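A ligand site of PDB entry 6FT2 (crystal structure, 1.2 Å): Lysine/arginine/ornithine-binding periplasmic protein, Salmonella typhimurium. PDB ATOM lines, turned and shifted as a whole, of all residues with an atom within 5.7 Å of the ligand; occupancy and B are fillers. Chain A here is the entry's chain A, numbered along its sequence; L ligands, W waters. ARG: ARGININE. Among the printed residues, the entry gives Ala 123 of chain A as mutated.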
ATOM      1  N   THR A  11      24.559  16.526   7.754  1.00  0.00           N
ATOM      2  CA  THR A  11      23.451  16.372   6.836  1.00  0.00           C
ATOM      3  C   THR A  11      22.232  15.912   7.623  1.00  0.00           C
ATOM      4  O   THR A  11      22.370  15.184   8.601  1.00  0.00           O
ATOM      5  CB  THR A  11      23.826  15.391   5.699  1.00  0.00           C
ATOM      6  OG1 THR A  11      22.872  15.507   4.622  1.00  0.00           O
ATOM      7  CG2 THR A  11      23.934  13.932   6.164  1.00  0.00           C
ATOM      8  N   ASP A  12      21.041  16.241   7.142  1.00  0.00           N
ATOM      9  CA  ASP A  12      19.803  15.724   7.707  1.00  0.00           C
ATOM     10  C   ASP A  12      19.343  14.613   6.741  1.00  0.00           C
ATOM     11  O   ASP A  12      19.007  14.869   5.582  1.00  0.00           O
ATOM     12  CB  ASP A  12      18.756  16.843   7.801  1.00  0.00           C
ATOM     13  CG  ASP A  12      17.331  16.391   7.944  1.00  0.00           C
ATOM     14  OD1 ASP A  12      17.111  15.296   8.473  1.00  0.00           O
ATOM     15  OD2 ASP A  12      16.442  17.214   7.726  1.00  0.00           O
ATOM     16  N   THR A  13      19.342  13.353   7.221  1.00  0.00           N
ATOM     17  CA  THR A  13      19.029  12.164   6.424  1.00  0.00           C
ATOM     18  C   THR A  13      17.554  11.843   6.318  1.00  0.00           C
ATOM     19  O   THR A  13      17.182  10.657   6.298  1.00  0.00           O
ATOM     20  CB  THR A  13      19.801  10.960   6.973  1.00  0.00           C
ATOM     21  OG1 THR A  13      19.374  10.730   8.300  1.00  0.00           O
ATOM     22  CG2 THR A  13      21.302  11.185   6.947  1.00  0.00           C
ATOM     23  N   THR A  14      16.707  12.856   6.153  1.00  0.00           N
ATOM     24  CA  THR A  14      15.287  12.602   5.944  1.00  0.00           C
ATOM     25  C   THR A  14      14.790  13.384   4.750  1.00  0.00           C
ATOM     26  O   THR A  14      13.658  13.855   4.735  1.00  0.00           O
ATOM     27  CB  THR A  14      14.448  12.932   7.216  1.00  0.00           C
ATOM     28  OG1 THR A  14      14.622  14.319   7.543  1.00  0.00           O
ATOM     29  CG2 THR A  14      14.846  12.102   8.427  1.00  0.00           C
ATOM     30  N   TYR A  15      15.619  13.474   3.701  1.00  0.00           N
ATOM     31  CA  TYR A  15      15.242  14.263   2.531  1.00  0.00           C
ATOM     32  C   TYR A  15      15.701  13.548   1.260  1.00  0.00           C
ATOM     33  O   TYR A  15      16.521  14.056   0.476  1.00  0.00           O
ATOM     34  CB  TYR A  15      15.888  15.683   2.645  1.00  0.00           C
ATOM     35  CG  TYR A  15      15.022  16.847   2.266  1.00  0.00           C
ATOM     36  CD1 TYR A  15      13.901  17.158   2.995  1.00  0.00           C
ATOM     37  CD2 TYR A  15      15.391  17.698   1.225  1.00  0.00           C
ATOM     38  CE1 TYR A  15      13.139  18.296   2.711  1.00  0.00           C
ATOM     39  CE2 TYR A  15      14.640  18.843   0.929  1.00  0.00           C
ATOM     40  CZ  TYR A  15      13.519  19.130   1.685  1.00  0.00           C
ATOM     41  OH  TYR A  15      12.790  20.276   1.470  1.00  0.00           O
ATOM     42  N   SER A  19      19.420  13.140   0.658  1.00  0.00           N
ATOM     43  CA  SER A  19      20.087  12.603   1.835  1.00  0.00           C
ATOM     44  C   SER A  19      19.086  11.767   2.597  1.00  0.00           C
ATOM     45  O   SER A  19      18.055  12.270   3.066  1.00  0.00           O
ATOM     46  CB  SER A  19      20.603  13.742   2.709  1.00  0.00           C
ATOM     47  OG  SER A  19      21.328  13.241   3.822  1.00  0.00           O
ATOM     48  N   ASP A  31      23.211  14.276  -2.412  1.00  0.00           N
ATOM     49  CA  ASP A  31      24.104  15.114  -1.599  1.00  0.00           C
ATOM     50  C   ASP A  31      25.313  14.305  -1.139  1.00  0.00           C
ATOM     51  O   ASP A  31      26.419  14.800  -1.022  1.00  0.00           O
ATOM     52  CB  ASP A  31      23.363  15.630  -0.370  1.00  0.00           C
ATOM     53  CG  ASP A  31      22.585  16.893  -0.571  1.00  0.00           C
ATOM     54  OD1 ASP A  31      22.712  17.493  -1.651  1.00  0.00           O
ATOM     55  OD2 ASP A  31      21.842  17.271   0.364  1.00  0.00           O
ATOM     56  N   PHE A  53      17.762  19.006  10.704  1.00  0.00           N
ATOM     57  CA  PHE A  53      18.108  20.103   9.818  1.00  0.00           C
ATOM     58  C   PHE A  53      18.339  21.426  10.574  1.00  0.00           C
ATOM     59  O   PHE A  53      19.278  22.175  10.280  1.00  0.00           O
ATOM     60  CB  PHE A  53      17.025  20.244   8.761  1.00  0.00           C
ATOM     61  CG  PHE A  53      17.394  21.269   7.717  1.00  0.00           C
ATOM     62  CD1 PHE A  53      18.315  20.971   6.723  1.00  0.00           C
ATOM     63  CD2 PHE A  53      16.805  22.528   7.736  1.00  0.00           C
ATOM     64  CE1 PHE A  53      18.688  21.922   5.791  1.00  0.00           C
ATOM     65  CE2 PHE A  53      17.146  23.467   6.756  1.00  0.00           C
ATOM     66  CZ  PHE A  53      18.109  23.159   5.805  1.00  0.00           C
ATOM     67  N   SER A  70      23.216  19.388   2.677  1.00  0.00           N
ATOM     68  CA  SER A  70      21.893  18.943   3.124  1.00  0.00           C
ATOM     69  C   SER A  70      20.814  19.762   2.418  1.00  0.00           C
ATOM     70  O   SER A  70      19.920  20.296   3.081  1.00  0.00           O
ATOM     71  CB  SER A  70      21.803  19.186   4.636  1.00  0.00           C
ATOM     72  OG  SER A  70      20.818  18.391   5.273  1.00  0.00           O
ATOM     73  N   SER A  71      20.932  19.898   1.097  1.00  0.00           N
ATOM     74  CA  SER A  71      20.039  20.736   0.296  1.00  0.00           C
ATOM     75  C   SER A  71      19.893  22.123   0.875  1.00  0.00           C
ATOM     76  O   SER A  71      18.766  22.660   0.957  1.00  0.00           O
ATOM     77  CB  SER A  71      18.652  20.124   0.138  1.00  0.00           C
ATOM     78  OG  SER A  71      18.667  18.834  -0.460  1.00  0.00           O
ATOM     79  N   LEU A  72      21.052  22.691   1.312  1.00  0.00           N
ATOM     80  CA  LEU A  72      20.981  23.967   2.019  1.00  0.00           C
ATOM     81  C   LEU A  72      20.904  25.130   1.082  1.00  0.00           C
ATOM     82  O   LEU A  72      21.857  25.449   0.403  1.00  0.00           O
ATOM     83  CB  LEU A  72      22.208  24.078   2.923  1.00  0.00           C
ATOM     84  CG  LEU A  72      22.197  25.240   3.906  1.00  0.00           C
ATOM     85  CD1 LEU A  72      21.170  25.027   5.004  1.00  0.00           C
ATOM     86  CD2 LEU A  72      23.575  25.402   4.563  1.00  0.00           C
ATOM     87  N   SER A  73      19.710  25.738   1.003  1.00  0.00           N
ATOM     88  CA  SER A  73      19.503  26.849   0.074  1.00  0.00           C
ATOM     89  C   SER A  73      20.378  28.064   0.428  1.00  0.00           C
ATOM     90  O   SER A  73      20.546  28.422   1.611  1.00  0.00           O
ATOM     91  CB  SER A  73      18.032  27.257   0.069  1.00  0.00           C
ATOM     92  OG  SER A  73      17.209  26.232  -0.471  1.00  0.00           O
ATOM     93  N   ARG A  78      20.986  33.567   5.289  1.00  0.00           N
ATOM     94  CA  ARG A  78      22.062  32.667   5.684  1.00  0.00           C
ATOM     95  C   ARG A  78      23.438  33.193   5.307  1.00  0.00           C
ATOM     96  O   ARG A  78      24.379  32.946   6.078  1.00  0.00           O
ATOM     97  CB  ARG A  78      21.828  31.269   5.114  1.00  0.00           C
ATOM     98  CG  ARG A  78      20.663  30.570   5.775  1.00  0.00           C
ATOM     99  CD  ARG A  78      20.341  29.349   4.976  1.00  0.00           C
ATOM    100  NE  ARG A  78      19.223  28.636   5.577  1.00  0.00           N
ATOM    101  CZ  ARG A  78      18.497  27.722   4.943  1.00  0.00           C
ATOM    102  NH1 ARG A  78      18.777  27.412   3.689  1.00  0.00           N
ATOM    103  NH2 ARG A  78      17.521  27.089   5.569  1.00  0.00           N
ATOM    104  N   ALA A  91      16.779  24.473  -6.201  1.00  0.00           N
ATOM    105  CA  ALA A  91      15.735  24.041  -5.272  1.00  0.00           C
ATOM    106  C   ALA A  91      14.647  25.077  -5.217  1.00  0.00           C
ATOM    107  O   ALA A  91      14.936  26.260  -5.007  1.00  0.00           O
ATOM    108  CB  ALA A  91      16.292  23.799  -3.868  1.00  0.00           C
ATOM    109  N   LEU A 118       9.311  22.002   7.541  1.00  0.00           N
ATOM    110  CA  LEU A 118      10.471  21.524   8.290  1.00  0.00           C
ATOM    111  C   LEU A 118      11.067  22.622   9.161  1.00  0.00           C
ATOM    112  O   LEU A 118      11.318  23.702   8.655  1.00  0.00           O
ATOM    113  CB  LEU A 118      11.480  20.976   7.244  1.00  0.00           C
ATOM    114  CG  LEU A 118      12.853  20.647   7.801  1.00  0.00           C
ATOM    115  CD1 LEU A 118      12.781  19.461   8.771  1.00  0.00           C
ATOM    116  CD2 LEU A 118      13.768  20.296   6.645  1.00  0.00           C
ATOM    117  N   GLY A 120      13.531  25.075  10.693  1.00  0.00           N
ATOM    118  CA  GLY A 120      14.813  25.549  10.199  1.00  0.00           C
ATOM    119  C   GLY A 120      14.894  25.798   8.715  1.00  0.00           C
ATOM    120  O   GLY A 120      15.916  26.306   8.244  1.00  0.00           O
ATOM    121  N   SER A 121      13.813  25.448   7.960  1.00  0.00           N
ATOM    122  CA  SER A 121      13.825  25.549   6.507  1.00  0.00           C
ATOM    123  C   SER A 121      13.342  26.855   5.942  1.00  0.00           C
ATOM    124  O   SER A 121      12.660  27.624   6.629  1.00  0.00           O
ATOM    125  CB  SER A 121      12.990  24.407   5.916  1.00  0.00           C
ATOM    126  OG  SER A 121      11.599  24.623   6.164  1.00  0.00           O
ATOM    127  N   THR A 122      13.672  27.076   4.662  1.00  0.00           N
ATOM    128  CA  THR A 122      13.114  28.232   3.963  1.00  0.00           C
ATOM    129  C   THR A 122      11.559  28.101   3.873  1.00  0.00           C
ATOM    130  O   THR A 122      10.873  29.120   3.968  1.00  0.00           O
ATOM    131  CB  THR A 122      13.688  28.280   2.563  1.00  0.00           C
ATOM    132  OG1 THR A 122      13.433  27.027   1.956  1.00  0.00           O
ATOM    133  CG2 THR A 122      15.190  28.547   2.579  1.00  0.00           C
ATOM    134  N   ALA A 123      11.044  26.883   3.774  1.00  0.00           N
ATOM    135  CA  ALA A 123       9.582  26.677   3.751  1.00  0.00           C
ATOM    136  C   ALA A 123       8.943  27.188   5.040  1.00  0.00           C
ATOM    137  O   ALA A 123       7.872  27.814   5.025  1.00  0.00           O
ATOM    138  CB  ALA A 123       9.254  25.194   3.578  1.00  0.00           C
ATOM    139  N   GLN A 144      11.534  15.870   7.908  1.00  0.00           N
ATOM    140  CA  GLN A 144      10.531  15.790   6.832  1.00  0.00           C
ATOM    141  C   GLN A 144       9.789  14.461   6.832  1.00  0.00           C
ATOM    142  O   GLN A 144       8.668  14.379   6.320  1.00  0.00           O
ATOM    143  CB  GLN A 144      11.227  16.049   5.486  1.00  0.00           C
ATOM    144  CG  GLN A 144      10.309  16.103   4.290  1.00  0.00           C
ATOM    145  CD  GLN A 144       9.477  17.355   4.248  1.00  0.00           C
ATOM    146  OE1 GLN A 144       9.921  18.475   4.572  1.00  0.00           O
ATOM    147  NE2 GLN A 144       8.275  17.183   3.710  1.00  0.00           N
ATOM    148  N   ASP A 162      10.948  21.222  -0.560  1.00  0.00           N
ATOM    149  CA  ASP A 162      11.537  21.314  -1.868  1.00  0.00           C
ATOM    150  C   ASP A 162      10.816  20.402  -2.855  1.00  0.00           C
ATOM    151  O   ASP A 162      10.498  19.259  -2.547  1.00  0.00           O
ATOM    152  CB  ASP A 162      13.060  21.033  -1.815  1.00  0.00           C
ATOM    153  CG  ASP A 162      13.898  22.092  -1.141  1.00  0.00           C
ATOM    154  OD1 ASP A 162      13.333  23.167  -0.755  1.00  0.00           O
ATOM    155  OD2 ASP A 162      15.078  21.837  -0.895  1.00  0.00           O
ATOM    156  N   THR A 196      21.175  25.450  -3.900  1.00  0.00           N
ATOM    157  CA  THR A 196      21.735  24.937  -2.664  1.00  0.00           C
ATOM    158  C   THR A 196      23.241  24.972  -2.785  1.00  0.00           C
ATOM    159  O   THR A 196      23.777  25.000  -3.899  1.00  0.00           O
ATOM    160  CB  THR A 196      21.255  23.533  -2.365  1.00  0.00           C
ATOM    161  OG1 THR A 196      21.838  22.626  -3.302  1.00  0.00           O
ATOM    162  CG2 THR A 196      19.714  23.414  -2.366  1.00  0.00           C
HETATM  163  N   ARG L   1      16.277  23.857   0.768  1.00  0.00           N
HETATM  164  CA  ARG L   1      15.516  24.056   2.009  1.00  0.00           C
HETATM  165  C   ARG L   1      16.344  24.882   2.940  1.00  0.00           C
HETATM  166  O   ARG L   1      15.785  25.326   3.965  1.00  0.00           O
HETATM  167  CB  ARG L   1      15.131  22.712   2.660  1.00  0.00           C
HETATM  168  CG  ARG L   1      16.269  21.709   2.853  1.00  0.00           C
HETATM  169  CD  ARG L   1      16.037  20.533   3.827  1.00  0.00           C
HETATM  170  NE  ARG L   1      17.133  19.554   3.715  1.00  0.00           N
HETATM  171  CZ  ARG L   1      17.222  18.441   4.443  1.00  0.00           C
HETATM  172  NH1 ARG L   1      16.264  18.120   5.277  1.00  0.00           N
HETATM  173  NH2 ARG L   1      18.244  17.552   4.239  1.00  0.00           N
HETATM  174  OXT ARG L   1      17.512  25.132   2.623  1.00  0.00           O
HETATM  175  O   HOH W   1      14.110  16.657   6.733  1.00  0.00           O
HETATM  176  O   HOH W   2      11.900  21.833   3.461  1.00  0.00           O
HETATM  177  O   HOH W   3      19.310  16.989   1.613  1.00  0.00           O
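The backbone NH of Thr 122 sits at hydrogen-bond distance from an oxygen (O) of the ligand (2.8 Å).
The side-chain carboxylate (OD2) of Asp 162 is in salt-bridge range of a nitrogen (N) of the ligand, 2.9 Å away.
The guanidinium group (NH1) of Arg 78 lies within salt-bridge range of an oxygen (OXT) of the ligand (2.8 Å).
A nitrogen (NE) of the ligand lies within hydrogen-bond range of the backbone carbonyl oxygen (O) of Ser 70, 3.0 Å away.
OXT of the ligand sits at hydrogen-bond distance from N of Ser 73 (2.8 Å).
OD2 of Asp 12 lies within salt-bridge range of NH1 of the ligand (2.6 Å).
The backbone carbonyl oxygen (O) of Ser 71 lies within hydrogen-bond range of a nitrogen (N) of the ligand (2.8 Å).
NH2 of the ligand sits at hydrogen-bond distance from OG of Ser 70, 2.9 Å away.
A nitrogen (NH2) of the ligand is in hydrogen-bond range of the backbone carbonyl oxygen (O) of Asp 12, 3.1 Å away.
A nitrogen (N) of the ligand is in hydrogen-bond range of the side-chain hydroxyl of Ser 73, at 2.8 Å.
The backbone carbonyl oxygen of Asp 12 sits at hydrogen-bond distance from the side-chain hydroxyl of Ser 19, at 3.3 Å.
NH2 of Arg 78 is in hydrogen-bond range of O of Gly 120, at 3.2 Å.
O of Leu 118 is in hydrogen-bond range of OG of Ser 121 (2.7 Å).
The backbone NH (N) of Ser 70 lies close to the side-chain carboxylate (OD2) of Asp 31.
The side-chain hydroxyl (OG) of Ser 121 sits close to the backbone NH (N) of Ala 123 (3.3 Å).
The guanidinium group of Arg 78 is in hydrogen-bond range of the backbone carbonyl oxygen of Ser 73.
The side-chain carboxylate (OD1) of Asp 12 is in hydrogen-bond range of the side-chain hydroxyl (OG1) of Thr 14, 2.8 Å away.
N of Ser 71 lies within hydrogen-bond range of OD2 of Asp 31, 2.9 Å away.
CB of Tyr 15 touches NH2 of the ligand, 3.4 Å away.
CE1 of Phe 53 touches NE of the ligand, 3.5 Å away.
Leu 72 touches the ligand.
Leu 118 touches the ligand (CD2 to NH1, 3.6 Å).
Ser 121 touches the ligand (CA to O, 3.2 Å).
Hydrophobic or aromatic side chains within 4 Å of the ligand: Tyr 15, Phe 53 and Leu 118.
12 residues have an atom within 4 Å of the ligand: Asp 12, Tyr 15, Phe 53, Ser 70, Ser 71, Leu 72, Ser 73, Arg 78, Leu 118, Ser 121, Thr 122 and Asp 162.
Water W3 lies within hydrogen-bond range of OD2 of Asp 31 (2.8 Å), OG of Ser 71 (2.8 Å) and NH2 of the ligand (2.9 Å).
Water W1 lies within hydrogen-bond range of OG1 of Thr 14 (2.5 Å), OD2 of Asp 12 (2.6 Å), N of Gln 144 (2.9 Å) and NH1 of the ligand (3.0 Å).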
